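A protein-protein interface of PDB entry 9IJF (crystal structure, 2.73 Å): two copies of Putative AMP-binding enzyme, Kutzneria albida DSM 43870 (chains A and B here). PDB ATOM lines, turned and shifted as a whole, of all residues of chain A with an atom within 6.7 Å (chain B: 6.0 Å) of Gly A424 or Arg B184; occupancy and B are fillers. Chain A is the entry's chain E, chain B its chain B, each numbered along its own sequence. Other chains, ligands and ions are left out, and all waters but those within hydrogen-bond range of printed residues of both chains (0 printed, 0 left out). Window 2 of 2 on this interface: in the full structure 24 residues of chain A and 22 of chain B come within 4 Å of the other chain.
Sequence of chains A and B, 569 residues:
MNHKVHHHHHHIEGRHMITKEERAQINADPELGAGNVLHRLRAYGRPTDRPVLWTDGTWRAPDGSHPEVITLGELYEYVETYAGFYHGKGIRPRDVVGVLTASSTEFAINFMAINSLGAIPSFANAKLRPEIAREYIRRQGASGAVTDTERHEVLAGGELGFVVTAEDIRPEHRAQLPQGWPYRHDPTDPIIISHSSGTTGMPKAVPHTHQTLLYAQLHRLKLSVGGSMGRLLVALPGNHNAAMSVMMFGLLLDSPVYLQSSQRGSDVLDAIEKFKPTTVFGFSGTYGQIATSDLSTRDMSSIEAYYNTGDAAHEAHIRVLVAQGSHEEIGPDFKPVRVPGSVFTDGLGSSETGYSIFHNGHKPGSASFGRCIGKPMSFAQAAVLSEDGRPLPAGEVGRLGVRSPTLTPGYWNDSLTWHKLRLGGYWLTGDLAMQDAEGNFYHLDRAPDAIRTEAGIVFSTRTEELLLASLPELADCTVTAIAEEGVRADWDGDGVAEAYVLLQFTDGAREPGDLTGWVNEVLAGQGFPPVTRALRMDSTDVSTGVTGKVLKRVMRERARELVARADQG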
ATOM      1  N   LEU A 385     -17.374   5.083  -5.962  1.00  0.00           N
ATOM      2  CA  LEU A 385     -17.622   5.294  -4.548  1.00  0.00           C
ATOM      3  C   LEU A 385     -18.541   4.236  -3.961  1.00  0.00           C
ATOM      4  O   LEU A 385     -19.543   3.866  -4.574  1.00  0.00           O
ATOM      5  CB  LEU A 385     -18.236   6.676  -4.317  1.00  0.00           C
ATOM      6  CG  LEU A 385     -17.387   7.899  -4.644  1.00  0.00           C
ATOM      7  CD1 LEU A 385     -18.286   9.138  -4.613  1.00  0.00           C
ATOM      8  CD2 LEU A 385     -16.252   8.017  -3.660  1.00  0.00           C
ATOM      9  N   ASP A 388     -21.110   4.742   1.362  1.00  0.00           N
ATOM     10  CA  ASP A 388     -20.769   5.683   2.421  1.00  0.00           C
ATOM     11  C   ASP A 388     -19.688   6.669   1.994  1.00  0.00           C
ATOM     12  O   ASP A 388     -19.038   7.275   2.855  1.00  0.00           O
ATOM     13  CB  ASP A 388     -20.340   4.948   3.697  1.00  0.00           C
ATOM     14  CG  ASP A 388     -18.927   4.357   3.604  1.00  0.00           C
ATOM     15  OD1 ASP A 388     -18.717   3.368   2.852  1.00  0.00           O
ATOM     16  OD2 ASP A 388     -18.018   4.885   4.287  1.00  0.00           O
ATOM     17  N   GLY A 389     -19.472   6.834   0.687  1.00  0.00           N
ATOM     18  CA  GLY A 389     -18.669   7.932   0.180  1.00  0.00           C
ATOM     19  C   GLY A 389     -17.177   7.693   0.078  1.00  0.00           C
ATOM     20  O   GLY A 389     -16.406   8.657  -0.052  1.00  0.00           O
ATOM     21  N   ARG A 390     -16.743   6.447   0.075  1.00  0.00           N
ATOM     22  CA  ARG A 390     -15.334   6.149   0.164  1.00  0.00           C
ATOM     23  C   ARG A 390     -14.875   5.364  -1.068  1.00  0.00           C
ATOM     24  O   ARG A 390     -15.555   4.408  -1.482  1.00  0.00           O
ATOM     25  CB  ARG A 390     -15.130   5.386   1.485  1.00  0.00           C
ATOM     26  CG  ARG A 390     -13.927   4.561   1.695  1.00  0.00           C
ATOM     27  CD  ARG A 390     -14.112   3.924   3.084  1.00  0.00           C
ATOM     28  NE  ARG A 390     -14.435   4.925   4.108  1.00  0.00           N
ATOM     29  CZ  ARG A 390     -14.989   4.666   5.292  1.00  0.00           C
ATOM     30  NH1 ARG A 390     -15.404   3.451   5.618  1.00  0.00           N
ATOM     31  NH2 ARG A 390     -15.126   5.651   6.176  1.00  0.00           N
ATOM     32  N   PRO A 391     -13.789   5.776  -1.730  1.00  0.00           N
ATOM     33  CA  PRO A 391     -13.425   5.152  -3.016  1.00  0.00           C
ATOM     34  C   PRO A 391     -13.140   3.662  -2.880  1.00  0.00           C
ATOM     35  O   PRO A 391     -12.520   3.212  -1.915  1.00  0.00           O
ATOM     36  CB  PRO A 391     -12.173   5.927  -3.451  1.00  0.00           C
ATOM     37  CG  PRO A 391     -12.297   7.261  -2.776  1.00  0.00           C
ATOM     38  CD  PRO A 391     -13.004   6.992  -1.456  1.00  0.00           C
ATOM     39  N   ARG A 403     -14.729  15.248  -8.664  1.00  0.00           N
ATOM     40  CA  ARG A 403     -14.346  16.576  -8.202  1.00  0.00           C
ATOM     41  C   ARG A 403     -13.629  17.296  -9.324  1.00  0.00           C
ATOM     42  O   ARG A 403     -12.862  16.691 -10.073  1.00  0.00           O
ATOM     43  CB  ARG A 403     -13.435  16.528  -6.990  1.00  0.00           C
ATOM     44  CG  ARG A 403     -14.052  15.856  -5.821  1.00  0.00           C
ATOM     45  CD  ARG A 403     -13.069  15.755  -4.730  1.00  0.00           C
ATOM     46  NE  ARG A 403     -13.697  15.169  -3.559  1.00  0.00           N
ATOM     47  CZ  ARG A 403     -13.039  14.535  -2.600  1.00  0.00           C
ATOM     48  NH1 ARG A 403     -11.731  14.349  -2.675  1.00  0.00           N
ATOM     49  NH2 ARG A 403     -13.713  14.072  -1.547  1.00  0.00           N
ATOM     50  N   ARG A 422     -24.529  14.648  -4.164  1.00  0.00           N
ATOM     51  CA  ARG A 422     -23.165  14.683  -3.688  1.00  0.00           C
ATOM     52  C   ARG A 422     -22.977  13.583  -2.655  1.00  0.00           C
ATOM     53  O   ARG A 422     -23.901  13.254  -1.896  1.00  0.00           O
ATOM     54  CB  ARG A 422     -22.820  16.041  -3.079  1.00  0.00           C
ATOM     55  CG  ARG A 422     -22.735  17.198  -4.062  1.00  0.00           C
ATOM     56  CD  ARG A 422     -22.526  18.490  -3.327  1.00  0.00           C
ATOM     57  NE  ARG A 422     -21.556  18.299  -2.260  1.00  0.00           N
ATOM     58  CZ  ARG A 422     -20.262  18.566  -2.374  1.00  0.00           C
ATOM     59  NH1 ARG A 422     -19.757  19.091  -3.482  1.00  0.00           N
ATOM     60  NH2 ARG A 422     -19.457  18.314  -1.350  1.00  0.00           N
ATOM     61  N   LEU A 423     -21.761  13.035  -2.627  1.00  0.00           N
ATOM     62  CA  LEU A 423     -21.418  11.894  -1.795  1.00  0.00           C
ATOM     63  C   LEU A 423     -19.904  11.905  -1.559  1.00  0.00           C
ATOM     64  O   LEU A 423     -19.120  12.025  -2.519  1.00  0.00           O
ATOM     65  CB  LEU A 423     -21.862  10.599  -2.485  1.00  0.00           C
ATOM     66  CG  LEU A 423     -21.604   9.297  -1.749  1.00  0.00           C
ATOM     67  CD1 LEU A 423     -22.134   9.401  -0.355  1.00  0.00           C
ATOM     68  CD2 LEU A 423     -22.265   8.169  -2.476  1.00  0.00           C
ATOM     69  N   GLY A 424     -19.502  11.796  -0.288  1.00  0.00           N
ATOM     70  CA  GLY A 424     -18.113  11.850   0.114  1.00  0.00           C
ATOM     71  C   GLY A 424     -17.272  12.928  -0.550  1.00  0.00           C
ATOM     72  O   GLY A 424     -16.089  12.705  -0.859  1.00  0.00           O
ATOM     73  N   GLY A 425     -17.861  14.095  -0.785  1.00  0.00           N
ATOM     74  CA  GLY A 425     -17.149  15.174  -1.429  1.00  0.00           C
ATOM     75  C   GLY A 425     -17.228  15.211  -2.941  1.00  0.00           C
ATOM     76  O   GLY A 425     -16.801  16.208  -3.534  1.00  0.00           O
ATOM     77  N   TYR A 426     -17.755  14.169  -3.593  1.00  0.00           N
ATOM     78  CA  TYR A 426     -17.840  14.164  -5.049  1.00  0.00           C
ATOM     79  C   TYR A 426     -19.254  14.528  -5.493  1.00  0.00           C
ATOM     80  O   TYR A 426     -20.210  14.393  -4.734  1.00  0.00           O
ATOM     81  CB  TYR A 426     -17.444  12.801  -5.627  1.00  0.00           C
ATOM     82  CG  TYR A 426     -16.042  12.339  -5.305  1.00  0.00           C
ATOM     83  CD1 TYR A 426     -15.752  11.791  -4.059  1.00  0.00           C
ATOM     84  CD2 TYR A 426     -15.001  12.438  -6.255  1.00  0.00           C
ATOM     85  CE1 TYR A 426     -14.480  11.372  -3.738  1.00  0.00           C
ATOM     86  CE2 TYR A 426     -13.703  12.004  -5.945  1.00  0.00           C
ATOM     87  CZ  TYR A 426     -13.451  11.467  -4.672  1.00  0.00           C
ATOM     88  OH  TYR A 426     -12.194  11.017  -4.304  1.00  0.00           O
ATOM     89  N   ASN B  36     -19.984  15.041  14.058  1.00  0.00           N
ATOM     90  CA  ASN B  36     -19.707  13.771  14.729  1.00  0.00           C
ATOM     91  C   ASN B  36     -18.946  13.909  16.043  1.00  0.00           C
ATOM     92  O   ASN B  36     -18.329  12.926  16.471  1.00  0.00           O
ATOM     93  CB  ASN B  36     -18.894  12.790  13.830  1.00  0.00           C
ATOM     94  CG  ASN B  36     -17.545  13.369  13.391  1.00  0.00           C
ATOM     95  OD1 ASN B  36     -16.992  14.244  14.044  1.00  0.00           O
ATOM     96  ND2 ASN B  36     -17.030  12.891  12.272  1.00  0.00           N
ATOM     97  N   ARG B  94     -29.261  13.621   3.787  1.00  0.00           N
ATOM     98  CA  ARG B  94     -29.601  14.853   3.061  1.00  0.00           C
ATOM     99  C   ARG B  94     -31.095  15.217   3.088  1.00  0.00           C
ATOM    100  O   ARG B  94     -31.533  16.041   2.282  1.00  0.00           O
ATOM    101  CB  ARG B  94     -29.142  14.796   1.606  1.00  0.00           C
ATOM    102  CG  ARG B  94     -27.759  14.208   1.405  1.00  0.00           C
ATOM    103  CD  ARG B  94     -26.673  15.243   1.532  1.00  0.00           C
ATOM    104  NE  ARG B  94     -25.418  14.670   1.086  1.00  0.00           N
ATOM    105  CZ  ARG B  94     -24.541  14.113   1.905  1.00  0.00           C
ATOM    106  NH1 ARG B  94     -24.710  14.152   3.220  1.00  0.00           N
ATOM    107  NH2 ARG B  94     -23.473  13.499   1.396  1.00  0.00           N
ATOM    108  N   PRO B 182     -22.856   5.530  13.162  1.00  0.00           N
ATOM    109  CA  PRO B 182     -23.358   6.817  12.655  1.00  0.00           C
ATOM    110  C   PRO B 182     -22.772   7.235  11.299  1.00  0.00           C
ATOM    111  O   PRO B 182     -21.868   6.577  10.779  1.00  0.00           O
ATOM    112  CB  PRO B 182     -22.924   7.775  13.766  1.00  0.00           C
ATOM    113  CG  PRO B 182     -21.562   7.239  14.137  1.00  0.00           C
ATOM    114  CD  PRO B 182     -21.645   5.725  13.971  1.00  0.00           C
ATOM    115  N   TYR B 183     -23.237   8.363  10.754  1.00  0.00           N
ATOM    116  CA  TYR B 183     -22.864   8.801   9.411  1.00  0.00           C
ATOM    117  C   TYR B 183     -21.431   9.343   9.355  1.00  0.00           C
ATOM    118  O   TYR B 183     -20.971  10.027  10.277  1.00  0.00           O
ATOM    119  CB  TYR B 183     -23.850   9.876   8.954  1.00  0.00           C
ATOM    120  CG  TYR B 183     -23.857  10.184   7.473  1.00  0.00           C
ATOM    121  CD1 TYR B 183     -24.549   9.375   6.580  1.00  0.00           C
ATOM    122  CD2 TYR B 183     -23.214  11.318   6.969  1.00  0.00           C
ATOM    123  CE1 TYR B 183     -24.572   9.657   5.210  1.00  0.00           C
ATOM    124  CE2 TYR B 183     -23.238  11.620   5.594  1.00  0.00           C
ATOM    125  CZ  TYR B 183     -23.915  10.783   4.719  1.00  0.00           C
ATOM    126  OH  TYR B 183     -23.949  11.066   3.360  1.00  0.00           O
ATOM    127  N   ARG B 184     -20.717   9.055   8.255  1.00  0.00           N
ATOM    128  CA  ARG B 184     -19.393   9.640   8.050  1.00  0.00           C
ATOM    129  C   ARG B 184     -19.559  10.831   7.109  1.00  0.00           C
ATOM    130  O   ARG B 184     -19.845  10.672   5.921  1.00  0.00           O
ATOM    131  CB  ARG B 184     -18.350   8.623   7.555  1.00  0.00           C
ATOM    132  CG  ARG B 184     -18.250   8.325   6.052  1.00  0.00           C
ATOM    133  CD  ARG B 184     -16.800   8.123   5.517  1.00  0.00           C
ATOM    134  NE  ARG B 184     -16.188   9.332   4.956  1.00  0.00           N
ATOM    135  CZ  ARG B 184     -16.554   9.915   3.813  1.00  0.00           C
ATOM    136  NH1 ARG B 184     -17.538   9.428   3.071  1.00  0.00           N
ATOM    137  NH2 ARG B 184     -15.923  11.025   3.412  1.00  0.00           N
ATOM    138  N   HIS B 185     -19.424  12.034   7.659  1.00  0.00           N
ATOM    139  CA  HIS B 185     -19.598  13.239   6.867  1.00  0.00           C
ATOM    140  C   HIS B 185     -18.341  13.563   6.073  1.00  0.00           C
ATOM    141  O   HIS B 185     -17.219  13.427   6.564  1.00  0.00           O
ATOM    142  CB  HIS B 185     -19.939  14.426   7.765  1.00  0.00           C
ATOM    143  CG  HIS B 185     -21.231  14.274   8.493  1.00  0.00           C
ATOM    144  ND1 HIS B 185     -21.309  13.744   9.762  1.00  0.00           N
ATOM    145  CD2 HIS B 185     -22.502  14.547   8.116  1.00  0.00           C
ATOM    146  CE1 HIS B 185     -22.574  13.713  10.141  1.00  0.00           C
ATOM    147  NE2 HIS B 185     -23.316  14.193   9.160  1.00  0.00           N
ATOM    148  N   ASP B 186     -18.534  14.001   4.837  1.00  0.00           N
ATOM    149  CA  ASP B 186     -17.476  14.739   4.195  1.00  0.00           C
ATOM    150  C   ASP B 186     -17.357  16.109   4.866  1.00  0.00           C
ATOM    151  O   ASP B 186     -18.347  16.626   5.387  1.00  0.00           O
ATOM    152  CB  ASP B 186     -17.762  14.902   2.706  1.00  0.00           C
ATOM    153  CG  ASP B 186     -16.541  15.347   1.948  1.00  0.00           C
ATOM    154  OD1 ASP B 186     -15.620  14.503   1.802  1.00  0.00           O
ATOM    155  OD2 ASP B 186     -16.469  16.543   1.553  1.00  0.00           O
ATOM    156  N   PRO B 187     -16.138  16.720   4.884  1.00  0.00           N
ATOM    157  CA  PRO B 187     -16.026  18.142   5.252  1.00  0.00           C
ATOM    158  C   PRO B 187     -17.179  18.998   4.732  1.00  0.00           C
ATOM    159  O   PRO B 187     -17.721  19.845   5.451  1.00  0.00           O
ATOM    160  CB  PRO B 187     -14.695  18.558   4.605  1.00  0.00           C
ATOM    161  CG  PRO B 187     -13.876  17.335   4.658  1.00  0.00           C
ATOM    162  CD  PRO B 187     -14.819  16.149   4.549  1.00  0.00           C
ATOM    163  N   THR B 188     -17.584  18.740   3.492  1.00  0.00           N
ATOM    164  CA  THR B 188     -18.507  19.589   2.756  1.00  0.00           C
ATOM    165  C   THR B 188     -19.973  19.246   2.985  1.00  0.00           C
ATOM    166  O   THR B 188     -20.833  19.903   2.397  1.00  0.00           O
ATOM    167  CB  THR B 188     -18.185  19.505   1.255  1.00  0.00           C
ATOM    168  OG1 THR B 188     -18.121  18.129   0.859  1.00  0.00           O
ATOM    169  CG2 THR B 188     -16.827  20.146   0.955  1.00  0.00           C
ATOM    170  N   ASP B 189     -20.283  18.260   3.828  1.00  0.00           N
ATOM    171  CA  ASP B 189     -21.665  17.798   3.987  1.00  0.00           C
ATOM    172  C   ASP B 189     -22.425  18.727   4.925  1.00  0.00           C
ATOM    173  O   ASP B 189     -21.929  19.033   6.010  1.00  0.00           O
ATOM    174  CB  ASP B 189     -21.713  16.354   4.512  1.00  0.00           C
ATOM    175  CG  ASP B 189     -21.476  15.315   3.404  1.00  0.00           C
ATOM    176  OD1 ASP B 189     -21.665  15.647   2.215  1.00  0.00           O
ATOM    177  OD2 ASP B 189     -21.096  14.159   3.707  1.00  0.00           O
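Arg A390 touches Arg B184. Gly A424 touches Arg B184 (CA to NH1, 3.9 Å). CA of Gly A425 touches OG1 of Thr B188 (3.9 Å).
Of the printed residues of chain B, Asp A388 touches Arg B184 (2.6 Å). Printed residues of chain B within 4 Å of Arg A390: Arg B184. Gly A424 touches just these residues of chain B: Arg B184 (3.9 Å) and Asp B186 (3.2 Å). Arg B184 touches just these residues of chain A: Asp A388 (2.6 Å), Gly A389 (3.4 Å), Arg A390 (3.1 Å) and Gly A424 (3.9 Å). The nearest residue of chain A that does not touch Arg B184 is Gly A425 (5.5 Å).
The guanidinium group (NH2) of Arg B94 lies within hydrogen-bond range of the backbone carbonyl oxygen (O) of Arg A422 (3.3 Å). O of Asp A388 is in hydrogen-bond range of NH1 of Arg B184. NH1 of Arg B184 is in hydrogen-bond range of O of Gly A389 (3.4 Å). The side-chain carboxylate (OD1) of Asp B186 is in salt-bridge range of the guanidinium group (NH2) of Arg A403. The backbone NH (N) of Gly A425 sits close to the side-chain carboxylate (OD1) of Asp B186 (3.4 Å). NH2 of Arg A422 lies within hydrogen-bond range of OG1 of Thr B188 (2.6 Å). The backbone carbonyl oxygen of Gly A424 sits close to the side-chain carboxylate of Asp B186 (3.2 Å).
OH of Tyr B183 sits at hydrogen-bond distance from NH2 of Arg B94. NH2 of Arg B184 is in salt-bridge range of OD1 of Asp B186 (3.8 Å). The backbone NH of Asp B186 is in hydrogen-bond range of the side-chain carboxylate of Asp B189 (2.8 Å). The side-chain carboxylate (OD2) of Asp A388 is in salt-bridge range of the guanidinium group (NH1) of Arg A390, 3.3 Å away. The backbone carbonyl oxygen (O) of Gly A424 is in hydrogen-bond range of the guanidinium group (NH2) of Arg A403 (2.8 Å). The guanidinium group (NE) of Arg A403 lies within hydrogen-bond range of the backbone carbonyl oxygen (O) of Gly A425 (3.3 Å).
Among the printed residues, 10 pairs touch across the chains.
No position is printed for both chains.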
